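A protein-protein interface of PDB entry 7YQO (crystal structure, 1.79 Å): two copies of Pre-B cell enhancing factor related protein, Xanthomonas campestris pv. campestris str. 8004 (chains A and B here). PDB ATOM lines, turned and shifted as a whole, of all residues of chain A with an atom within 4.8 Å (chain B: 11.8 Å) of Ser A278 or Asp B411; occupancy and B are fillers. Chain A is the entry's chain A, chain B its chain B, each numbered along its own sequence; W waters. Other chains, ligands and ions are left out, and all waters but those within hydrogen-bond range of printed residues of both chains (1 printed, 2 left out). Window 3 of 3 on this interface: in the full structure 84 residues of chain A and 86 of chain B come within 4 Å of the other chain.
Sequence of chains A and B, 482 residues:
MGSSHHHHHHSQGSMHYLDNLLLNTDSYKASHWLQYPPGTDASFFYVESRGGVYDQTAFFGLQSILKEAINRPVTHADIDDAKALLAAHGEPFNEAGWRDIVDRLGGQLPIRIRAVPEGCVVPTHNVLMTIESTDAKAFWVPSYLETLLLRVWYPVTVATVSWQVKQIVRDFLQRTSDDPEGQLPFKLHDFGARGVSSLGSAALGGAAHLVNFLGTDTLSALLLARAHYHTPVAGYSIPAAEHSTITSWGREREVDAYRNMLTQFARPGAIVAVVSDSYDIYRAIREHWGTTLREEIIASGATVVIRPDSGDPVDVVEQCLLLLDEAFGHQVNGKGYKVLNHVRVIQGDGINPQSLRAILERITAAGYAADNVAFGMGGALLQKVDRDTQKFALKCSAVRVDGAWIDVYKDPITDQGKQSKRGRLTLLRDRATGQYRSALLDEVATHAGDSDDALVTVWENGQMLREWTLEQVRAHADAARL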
ATOM      1  N   HIS A 243       7.386  24.988  15.667  1.00  0.00           N
ATOM      2  CA  HIS A 243       6.462  24.434  16.654  1.00  0.00           C
ATOM      3  C   HIS A 243       5.020  24.482  16.178  1.00  0.00           C
ATOM      4  O   HIS A 243       4.270  23.520  16.368  1.00  0.00           O
ATOM      5  CB  HIS A 243       6.579  25.169  17.978  1.00  0.00           C
ATOM      6  CG  HIS A 243       7.912  24.993  18.625  1.00  0.00           C
ATOM      7  ND1 HIS A 243       8.316  23.794  19.168  1.00  0.00           N
ATOM      8  CD2 HIS A 243       8.941  25.856  18.794  1.00  0.00           C
ATOM      9  CE1 HIS A 243       9.531  23.932  19.673  1.00  0.00           C
ATOM     10  NE2 HIS A 243       9.936  25.171  19.455  1.00  0.00           N
ATOM     11  N   ILE A 246       3.912  21.628  13.921  1.00  0.00           N
ATOM     12  CA  ILE A 246       3.866  20.342  14.621  1.00  0.00           C
ATOM     13  C   ILE A 246       2.653  20.279  15.545  1.00  0.00           C
ATOM     14  O   ILE A 246       1.879  19.313  15.531  1.00  0.00           O
ATOM     15  CB  ILE A 246       5.163  20.104  15.416  1.00  0.00           C
ATOM     16  CG1 ILE A 246       6.401  20.111  14.497  1.00  0.00           C
ATOM     17  CG2 ILE A 246       5.045  18.791  16.245  1.00  0.00           C
ATOM     18  CD1 ILE A 246       6.326  19.103  13.377  1.00  0.00           C
ATOM     19  N   THR A 247       2.500  21.291  16.402  1.00  0.00           N
ATOM     20  CA  THR A 247       1.461  21.230  17.423  1.00  0.00           C
ATOM     21  C   THR A 247       0.064  21.418  16.844  1.00  0.00           C
ATOM     22  O   THR A 247      -0.912  21.027  17.495  1.00  0.00           O
ATOM     23  CB  THR A 247       1.738  22.269  18.522  1.00  0.00           C
ATOM     24  OG1 THR A 247       1.764  23.585  17.939  1.00  0.00           O
ATOM     25  CG2 THR A 247       3.077  21.995  19.186  1.00  0.00           C
ATOM     26  N   ARG A 251      -1.298  16.663  20.080  1.00  0.00           N
ATOM     27  CA  ARG A 251      -0.322  15.840  20.794  1.00  0.00           C
ATOM     28  C   ARG A 251      -0.331  14.385  20.319  1.00  0.00           C
ATOM     29  O   ARG A 251       0.725  13.757  20.163  1.00  0.00           O
ATOM     30  CB  ARG A 251      -0.637  15.928  22.295  1.00  0.00           C
ATOM     31  CG  ARG A 251       0.280  15.168  23.206  1.00  0.00           C
ATOM     32  CD  ARG A 251      -0.203  15.277  24.660  1.00  0.00           C
ATOM     33  NE  ARG A 251      -0.278  16.662  25.138  1.00  0.00           N
ATOM     34  CZ  ARG A 251       0.677  17.264  25.848  1.00  0.00           C
ATOM     35  NH1 ARG A 251       1.794  16.616  26.151  1.00  0.00           N
ATOM     36  NH2 ARG A 251       0.522  18.523  26.242  1.00  0.00           N
ATOM     37  N   VAL A 275      12.293  20.716  14.762  1.00  0.00           N
ATOM     38  CA  VAL A 275      12.265  21.024  16.185  1.00  0.00           C
ATOM     39  C   VAL A 275      11.483  19.933  16.906  1.00  0.00           C
ATOM     40  O   VAL A 275      10.385  19.553  16.486  1.00  0.00           O
ATOM     41  CB  VAL A 275      11.686  22.428  16.412  1.00  0.00           C
ATOM     42  CG1 VAL A 275      10.181  22.485  16.036  1.00  0.00           C
ATOM     43  CG2 VAL A 275      11.956  22.855  17.846  1.00  0.00           C
ATOM     44  N   SER A 276      12.068  19.370  17.968  1.00  0.00           N
ATOM     45  CA  SER A 276      11.527  18.125  18.496  1.00  0.00           C
ATOM     46  C   SER A 276      11.080  18.216  19.951  1.00  0.00           C
ATOM     47  O   SER A 276      10.804  17.178  20.563  1.00  0.00           O
ATOM     48  CB  SER A 276      12.552  16.989  18.335  1.00  0.00           C
ATOM     49  OG  SER A 276      12.828  16.749  16.959  1.00  0.00           O
ATOM     50  N   ASP A 277      10.963  19.418  20.517  1.00  0.00           N
ATOM     51  CA  ASP A 277      10.577  19.575  21.919  1.00  0.00           C
ATOM     52  C   ASP A 277       9.175  20.159  22.081  1.00  0.00           C
ATOM     53  O   ASP A 277       8.905  20.850  23.071  1.00  0.00           O
ATOM     54  CB  ASP A 277      11.587  20.460  22.643  1.00  0.00           C
ATOM     55  CG  ASP A 277      11.475  21.911  22.213  1.00  0.00           C
ATOM     56  OD1 ASP A 277      11.113  22.120  21.042  1.00  0.00           O
ATOM     57  OD2 ASP A 277      11.717  22.832  23.031  1.00  0.00           O
ATOM     58  N   SER A 278       8.268  19.919  21.123  1.00  0.00           N
ATOM     59  CA  SER A 278       6.909  20.432  21.296  1.00  0.00           C
ATOM     60  C   SER A 278       6.279  19.898  22.570  1.00  0.00           C
ATOM     61  O   SER A 278       5.560  20.628  23.269  1.00  0.00           O
ATOM     62  CB  SER A 278       6.028  20.078  20.091  1.00  0.00           C
ATOM     63  OG  SER A 278       6.498  20.735  18.926  1.00  0.00           O
ATOM     64  N   TYR A 279       6.545  18.618  22.895  1.00  0.00           N
ATOM     65  CA  TYR A 279       5.921  17.967  24.044  1.00  0.00           C
ATOM     66  C   TYR A 279       6.931  17.327  24.983  1.00  0.00           C
ATOM     67  O   TYR A 279       6.769  17.422  26.206  1.00  0.00           O
ATOM     68  CB  TYR A 279       4.911  16.896  23.565  1.00  0.00           C
ATOM     69  CG  TYR A 279       3.880  17.455  22.614  1.00  0.00           C
ATOM     70  CD1 TYR A 279       2.877  18.290  23.073  1.00  0.00           C
ATOM     71  CD2 TYR A 279       3.917  17.156  21.256  1.00  0.00           C
ATOM     72  CE1 TYR A 279       1.927  18.823  22.202  1.00  0.00           C
ATOM     73  CE2 TYR A 279       2.968  17.687  20.373  1.00  0.00           C
ATOM     74  CZ  TYR A 279       1.981  18.522  20.855  1.00  0.00           C
ATOM     75  OH  TYR A 279       1.022  19.056  19.996  1.00  0.00           O
ATOM     76  N   ASP A 280       7.959  16.680  24.443  1.00  0.00           N
ATOM     77  CA  ASP A 280       8.945  15.937  25.226  1.00  0.00           C
ATOM     78  C   ASP A 280      10.024  15.455  24.274  1.00  0.00           C
ATOM     79  O   ASP A 280       9.824  14.473  23.549  1.00  0.00           O
ATOM     80  CB  ASP A 280       8.292  14.755  25.959  1.00  0.00           C
ATOM     81  CG  ASP A 280       9.285  13.952  26.828  1.00  0.00           C
ATOM     82  OD1 ASP A 280      10.500  13.951  26.559  1.00  0.00           O
ATOM     83  OD2 ASP A 280       8.840  13.298  27.796  1.00  0.00           O
ATOM     84  N   HIS B  32       6.920  26.039   4.582  1.00  0.00           N
ATOM     85  CA  HIS B  32       6.152  25.888   5.810  1.00  0.00           C
ATOM     86  C   HIS B  32       4.729  25.372   5.556  1.00  0.00           C
ATOM     87  O   HIS B  32       4.208  24.563   6.342  1.00  0.00           O
ATOM     88  CB  HIS B  32       6.226  27.250   6.515  1.00  0.00           C
ATOM     89  CG  HIS B  32       5.293  27.439   7.662  1.00  0.00           C
ATOM     90  ND1 HIS B  32       5.722  27.405   8.972  1.00  0.00           N
ATOM     91  CD2 HIS B  32       3.988  27.801   7.700  1.00  0.00           C
ATOM     92  CE1 HIS B  32       4.703  27.680   9.769  1.00  0.00           C
ATOM     93  NE2 HIS B  32       3.638  27.915   9.023  1.00  0.00           N
ATOM     94  N   GLN B  35       3.599  21.688   5.958  1.00  0.00           N
ATOM     95  CA  GLN B  35       3.771  21.049   7.256  1.00  0.00           C
ATOM     96  C   GLN B  35       2.503  20.989   8.092  1.00  0.00           C
ATOM     97  O   GLN B  35       2.501  20.292   9.116  1.00  0.00           O
ATOM     98  CB  GLN B  35       4.852  21.778   8.049  1.00  0.00           C
ATOM     99  CG  GLN B  35       6.159  21.919   7.280  1.00  0.00           C
ATOM    100  CD  GLN B  35       7.172  22.785   8.017  1.00  0.00           C
ATOM    101  OE1 GLN B  35       7.027  23.064   9.210  1.00  0.00           O
ATOM    102  NE2 GLN B  35       8.207  23.216   7.299  1.00  0.00           N
ATOM    103  N   LYS B 395       3.001  34.677  18.647  1.00  0.00           N
ATOM    104  CA  LYS B 395       2.727  33.250  18.763  1.00  0.00           C
ATOM    105  C   LYS B 395       1.469  32.884  18.001  1.00  0.00           C
ATOM    106  O   LYS B 395       0.505  33.642  18.000  1.00  0.00           O
ATOM    107  CB  LYS B 395       2.559  32.835  20.249  1.00  0.00           C
ATOM    108  CG  LYS B 395       3.872  32.901  21.060  1.00  0.00           C
ATOM    109  CD  LYS B 395       4.644  31.595  20.939  1.00  0.00           C
ATOM    110  CE  LYS B 395       6.118  31.767  21.306  1.00  0.00           C
ATOM    111  NZ  LYS B 395       6.836  30.465  21.095  1.00  0.00           N
ATOM    112  N   CYS B 396       1.472  31.705  17.378  1.00  0.00           N
ATOM    113  CA  CYS B 396       0.253  31.171  16.795  1.00  0.00           C
ATOM    114  C   CYS B 396      -0.539  30.572  17.941  1.00  0.00           C
ATOM    115  O   CYS B 396      -0.042  29.674  18.631  1.00  0.00           O
ATOM    116  CB  CYS B 396       0.577  30.102  15.750  1.00  0.00           C
ATOM    117  SG  CYS B 396      -0.939  29.361  14.963  1.00  0.00           S
ATOM    118  N   ASP B 407      -6.703  25.025  19.991  1.00  0.00           N
ATOM    119  CA  ASP B 407      -5.583  25.761  20.564  1.00  0.00           C
ATOM    120  C   ASP B 407      -4.267  25.160  20.085  1.00  0.00           C
ATOM    121  O   ASP B 407      -4.131  23.943  19.909  1.00  0.00           O
ATOM    122  CB  ASP B 407      -5.632  25.727  22.101  1.00  0.00           C
ATOM    123  CG  ASP B 407      -6.776  26.564  22.690  1.00  0.00           C
ATOM    124  OD1 ASP B 407      -7.416  27.359  21.954  1.00  0.00           O
ATOM    125  OD2 ASP B 407      -7.035  26.412  23.908  1.00  0.00           O
ATOM    126  N   VAL B 408      -3.280  26.028  19.898  1.00  0.00           N
ATOM    127  CA  VAL B 408      -1.952  25.650  19.438  1.00  0.00           C
ATOM    128  C   VAL B 408      -0.964  26.089  20.512  1.00  0.00           C
ATOM    129  O   VAL B 408      -0.982  27.259  20.911  1.00  0.00           O
ATOM    130  CB  VAL B 408      -1.629  26.328  18.090  1.00  0.00           C
ATOM    131  CG1 VAL B 408      -0.171  26.097  17.696  1.00  0.00           C
ATOM    132  CG2 VAL B 408      -2.590  25.805  16.994  1.00  0.00           C
ATOM    133  N   TYR B 409      -0.099  25.168  20.959  1.00  0.00           N
ATOM    134  CA  TYR B 409       0.829  25.448  22.060  1.00  0.00           C
ATOM    135  C   TYR B 409       1.786  24.285  22.267  1.00  0.00           C
ATOM    136  O   TYR B 409       1.417  23.116  22.092  1.00  0.00           O
ATOM    137  CB  TYR B 409       0.075  25.700  23.375  1.00  0.00           C
ATOM    138  CG  TYR B 409      -0.841  24.578  23.786  1.00  0.00           C
ATOM    139  CD1 TYR B 409      -2.140  24.501  23.283  1.00  0.00           C
ATOM    140  CD2 TYR B 409      -0.419  23.586  24.684  1.00  0.00           C
ATOM    141  CE1 TYR B 409      -2.983  23.475  23.639  1.00  0.00           C
ATOM    142  CE2 TYR B 409      -1.272  22.556  25.058  1.00  0.00           C
ATOM    143  CZ  TYR B 409      -2.545  22.509  24.531  1.00  0.00           C
ATOM    144  OH  TYR B 409      -3.408  21.502  24.880  1.00  0.00           O
ATOM    145  N   LYS B 410       2.996  24.611  22.713  1.00  0.00           N
ATOM    146  CA  LYS B 410       3.868  23.584  23.289  1.00  0.00           C
ATOM    147  C   LYS B 410       3.390  23.182  24.683  1.00  0.00           C
ATOM    148  O   LYS B 410       2.731  23.950  25.389  1.00  0.00           O
ATOM    149  CB  LYS B 410       5.307  24.082  23.413  1.00  0.00           C
ATOM    150  CG  LYS B 410       5.915  24.574  22.128  1.00  0.00           C
ATOM    151  CD  LYS B 410       7.400  24.240  22.079  1.00  0.00           C
ATOM    152  CE  LYS B 410       8.216  24.917  23.146  1.00  0.00           C
ATOM    153  NZ  LYS B 410       9.714  24.823  22.959  1.00  0.00           N
ATOM    154  N   ASP B 411       3.769  21.974  25.090  1.00  0.00           N
ATOM    155  CA  ASP B 411       3.499  21.538  26.454  1.00  0.00           C
ATOM    156  C   ASP B 411       4.105  22.525  27.452  1.00  0.00           C
ATOM    157  O   ASP B 411       5.209  23.026  27.228  1.00  0.00           O
ATOM    158  CB  ASP B 411       4.084  20.147  26.699  1.00  0.00           C
ATOM    159  CG  ASP B 411       3.620  19.562  28.012  1.00  0.00           C
ATOM    160  OD1 ASP B 411       4.265  19.813  29.056  1.00  0.00           O
ATOM    161  OD2 ASP B 411       2.584  18.876  28.003  1.00  0.00           O
ATOM    162  N   PRO B 412       3.415  22.823  28.563  1.00  0.00           N
ATOM    163  CA  PRO B 412       4.004  23.725  29.575  1.00  0.00           C
ATOM    164  C   PRO B 412       5.419  23.345  29.990  1.00  0.00           C
ATOM    165  O   PRO B 412       6.236  24.229  30.281  1.00  0.00           O
ATOM    166  CB  PRO B 412       3.030  23.603  30.753  1.00  0.00           C
ATOM    167  CG  PRO B 412       1.705  23.343  30.092  1.00  0.00           C
ATOM    168  CD  PRO B 412       2.013  22.482  28.872  1.00  0.00           C
ATOM    169  N   ILE B 413       5.750  22.053  29.991  1.00  0.00           N
ATOM    170  CA  ILE B 413       7.079  21.659  30.435  1.00  0.00           C
ATOM    171  C   ILE B 413       8.161  22.071  29.452  1.00  0.00           C
ATOM    172  O   ILE B 413       9.320  22.217  29.849  1.00  0.00           O
ATOM    173  CB  ILE B 413       7.116  20.145  30.729  1.00  0.00           C
ATOM    174  CG1 ILE B 413       8.093  19.873  31.874  1.00  0.00           C
ATOM    175  CG2 ILE B 413       7.487  19.335  29.493  1.00  0.00           C
ATOM    176  CD1 ILE B 413       8.300  18.431  32.168  1.00  0.00           C
ATOM    177  N   THR B 414       7.836  22.289  28.173  1.00  0.00           N
ATOM    178  CA  THR B 414       8.856  22.742  27.234  1.00  0.00           C
ATOM    179  C   THR B 414       8.667  24.185  26.790  1.00  0.00           C
ATOM    180  O   THR B 414       9.578  24.747  26.170  1.00  0.00           O
ATOM    181  CB  THR B 414       8.883  21.856  25.976  1.00  0.00           C
ATOM    182  OG1 THR B 414       7.618  21.958  25.321  1.00  0.00           O
ATOM    183  CG2 THR B 414       9.146  20.395  26.335  1.00  0.00           C
ATOM    184  N   ASP B 415       7.509  24.786  27.077  1.00  0.00           N
ATOM    185  CA  ASP B 415       7.223  26.129  26.600  1.00  0.00           C
ATOM    186  C   ASP B 415       8.058  27.194  27.298  1.00  0.00           C
ATOM    187  O   ASP B 415       8.261  28.268  26.724  1.00  0.00           O
ATOM    188  CB  ASP B 415       5.737  26.436  26.775  1.00  0.00           C
ATOM    189  CG  ASP B 415       5.343  27.759  26.143  1.00  0.00           C
ATOM    190  OD1 ASP B 415       5.600  27.927  24.922  1.00  0.00           O
ATOM    191  OD2 ASP B 415       4.785  28.632  26.855  1.00  0.00           O
ATOM    192  N   GLN B 416       8.534  26.928  28.517  1.00  0.00           N
ATOM    193  CA  GLN B 416       9.372  27.877  29.263  1.00  0.00           C
ATOM    194  C   GLN B 416       8.739  29.268  29.312  1.00  0.00           C
ATOM    195  O   GLN B 416       9.414  30.293  29.185  1.00  0.00           O
ATOM    196  CB  GLN B 416      10.787  27.908  28.679  1.00  0.00           C
ATOM    197  CG  GLN B 416      11.385  26.479  28.703  1.00  0.00           C
ATOM    198  CD  GLN B 416      12.896  26.414  28.544  1.00  0.00           C
ATOM    199  OE1 GLN B 416      13.551  25.532  29.116  1.00  0.00           O
ATOM    200  NE2 GLN B 416      13.456  27.323  27.757  1.00  0.00           N
ATOM    201  N   GLY B 417       7.416  29.291  29.471  1.00  0.00           N
ATOM    202  CA  GLY B 417       6.673  30.529  29.636  1.00  0.00           C
ATOM    203  C   GLY B 417       6.570  31.410  28.414  1.00  0.00           C
ATOM    204  O   GLY B 417       6.123  32.558  28.530  1.00  0.00           O
ATOM    205  N   LYS B 418       6.966  30.931  27.237  1.00  0.00           N
ATOM    206  CA  LYS B 418       6.994  31.837  26.093  1.00  0.00           C
ATOM    207  C   LYS B 418       5.616  32.078  25.483  1.00  0.00           C
ATOM    208  O   LYS B 418       5.449  33.061  24.753  1.00  0.00           O
ATOM    209  CB  LYS B 418       7.972  31.337  25.028  1.00  0.00           C
ATOM    210  CG  LYS B 418       9.342  30.976  25.621  1.00  0.00           C
ATOM    211  CD  LYS B 418      10.422  32.022  25.411  1.00  0.00           C
ATOM    212  CE  LYS B 418      11.673  31.705  26.271  1.00  0.00           C
ATOM    213  NZ  LYS B 418      11.471  31.829  27.767  1.00  0.00           N
ATOM    214  N   GLN B 419       4.623  31.246  25.779  1.00  0.00           N
ATOM    215  CA  GLN B 419       3.259  31.446  25.276  1.00  0.00           C
ATOM    216  C   GLN B 419       2.289  31.495  26.450  1.00  0.00           C
ATOM    217  O   GLN B 419       1.905  30.457  27.003  1.00  0.00           O
ATOM    218  CB  GLN B 419       2.855  30.348  24.298  1.00  0.00           C
ATOM    219  CG  GLN B 419       1.470  30.615  23.666  1.00  0.00           C
ATOM    220  CD  GLN B 419       1.067  29.566  22.643  1.00  0.00           C
ATOM    221  OE1 GLN B 419       1.915  28.829  22.129  1.00  0.00           O
ATOM    222  NE2 GLN B 419      -0.225  29.511  22.320  1.00  0.00           N
ATOM    223  N   SER B 420       1.851  32.691  26.806  1.00  0.00           N
ATOM    224  CA  SER B 420       0.952  32.835  27.939  1.00  0.00           C
ATOM    225  C   SER B 420      -0.515  32.683  27.574  1.00  0.00           C
ATOM    226  O   SER B 420      -1.345  32.575  28.484  1.00  0.00           O
ATOM    227  CB  SER B 420       1.162  34.205  28.608  1.00  0.00           C
ATOM    228  OG  SER B 420       0.777  35.257  27.737  1.00  0.00           O
ATOM    229  N   LYS B 421      -0.877  32.701  26.284  1.00  0.00           N
ATOM    230  CA  LYS B 421      -2.281  32.712  25.894  1.00  0.00           C
ATOM    231  C   LYS B 421      -2.537  31.717  24.767  1.00  0.00           C
ATOM    232  O   LYS B 421      -1.642  31.397  23.982  1.00  0.00           O
ATOM    233  CB  LYS B 421      -2.736  34.112  25.461  1.00  0.00           C
ATOM    234  CG  LYS B 421      -2.568  35.181  26.555  1.00  0.00           C
ATOM    235  CD  LYS B 421      -2.362  36.541  25.956  1.00  0.00           C
ATOM    236  CE  LYS B 421      -2.259  37.623  27.031  1.00  0.00           C
ATOM    237  NZ  LYS B 421      -1.269  37.313  28.092  1.00  0.00           N
ATOM    238  N   ARG B 422      -3.778  31.232  24.705  1.00  0.00           N
ATOM    239  CA  ARG B 422      -4.219  30.281  23.685  1.00  0.00           C
ATOM    240  C   ARG B 422      -5.571  30.720  23.133  1.00  0.00           C
ATOM    241  O   ARG B 422      -6.327  31.419  23.805  1.00  0.00           O
ATOM    242  CB  ARG B 422      -4.344  28.856  24.259  1.00  0.00           C
ATOM    243  CG  ARG B 422      -3.054  28.336  24.880  1.00  0.00           C
ATOM    244  CD  ARG B 422      -3.291  27.068  25.668  1.00  0.00           C
ATOM    245  NE  ARG B 422      -2.075  26.594  26.333  1.00  0.00           N
ATOM    246  CZ  ARG B 422      -2.028  25.504  27.094  1.00  0.00           C
ATOM    247  NH1 ARG B 422      -3.128  24.778  27.280  1.00  0.00           N
ATOM    248  NH2 ARG B 422      -0.890  25.136  27.663  1.00  0.00           N
HETATM  249  O   HOH W   1       4.969  16.395  28.077  1.00  0.00           O
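The side-chain carboxylate of Asp B411 lies within salt-bridge range of the guanidinium group of Arg A251 (2.7 Å).
OD2 of Asp A277 is in salt-bridge range of NZ of Lys B410, 2.8 Å away.
The side-chain hydroxyl of Thr B414 lies within hydrogen-bond range of the backbone carbonyl oxygen of Asp A277 (2.8 Å).
O of Ser A278 sits at hydrogen-bond distance from N of Asp B411 (2.9 Å).
The backbone carbonyl oxygen of Ser A278 sits at hydrogen-bond distance from the side-chain hydroxyl of Thr B414, 3.2 Å away.
No position is printed for both chains.
Of the 10 printed residues of chain A, 6 touch a printed residue of chain B.
Among the printed residues, Asp or Glu carboxylates within 4 Å of a Lys or Arg side-chain nitrogen of the other chain: Arg A251 with Asp B411 and Asp A277 with Lys B410.
Lys B410 touches His A243.
OG1 of Thr A247 touches CG1 of Val B408 (3.2 Å).
Tyr B409 touches Thr A247.
Lys B410 touches Ser A278.
Asp B411 touches Tyr A279.
Ile B413 touches Tyr A279.
CG2 of Thr B414 touches O of Tyr A279, at 3.8 Å.
His A243 touches just one residue of chain B: Lys B410 (3.1 Å).
Ile A246 touches none of the printed residues of chain B.
Of the printed residues of chain B, Thr A247 touches Val B408 (3.2 Å) and Tyr B409 (3.5 Å).
No residue of chain B comes within 4 Å of Val A275.
Asp A277 touches just these residues of chain B: Lys B410 and Thr B414.
Ser A278 touches just these residues of chain B: Lys B410, Asp B411 and Thr B414.
Of the printed residues of chain A, Lys B410 touches His A243 (3.1 Å), Asp A277 (2.8 Å) and Ser A278 (3.4 Å).
Asp B411 touches just these residues of chain A: Arg A251, Ser A278 and Tyr A279.
Of the printed residues of chain A, Thr B414 touches Asp A277 (2.8 Å), Ser A278 (3.2 Å) and Tyr A279 (3.8 Å).
Arg B422 touches none of the printed residues of chain A.
The nearest residue of chain B that does not touch Ser A278 is Tyr B409 (5.0 Å).
The nearest printed residue of chain A that does not touch Asp B411 is Asp A277 (5.6 Å).
The side-chain amino group (NZ) of Lys B410 lies within hydrogen-bond range of the backbone carbonyl oxygen (O) of Thr B414.
The backbone carbonyl oxygen of Val B408 is in hydrogen-bond range of the side-chain amide nitrogen of Gln B419.
The side-chain hydroxyl (OH) of Tyr A279 sits at hydrogen-bond distance from the backbone NH (N) of Arg A251, 3.3 Å away.
The backbone carbonyl oxygen (O) of Asp B411 sits at hydrogen-bond distance from the side-chain hydroxyl (OG1) of Thr B414, 3.3 Å away.
The backbone NH (N) of Ile B413 sits at hydrogen-bond distance from the side-chain carboxylate (OD1) of Asp B411 (2.8 Å).
The backbone carbonyl oxygen of His A243 lies within hydrogen-bond range of the side-chain hydroxyl of Thr A247 (3.0 Å).
Water W1 lies within hydrogen-bond range of O of Tyr A279 (2.8 Å) and OD2 of Asp B411 (3.4 Å).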
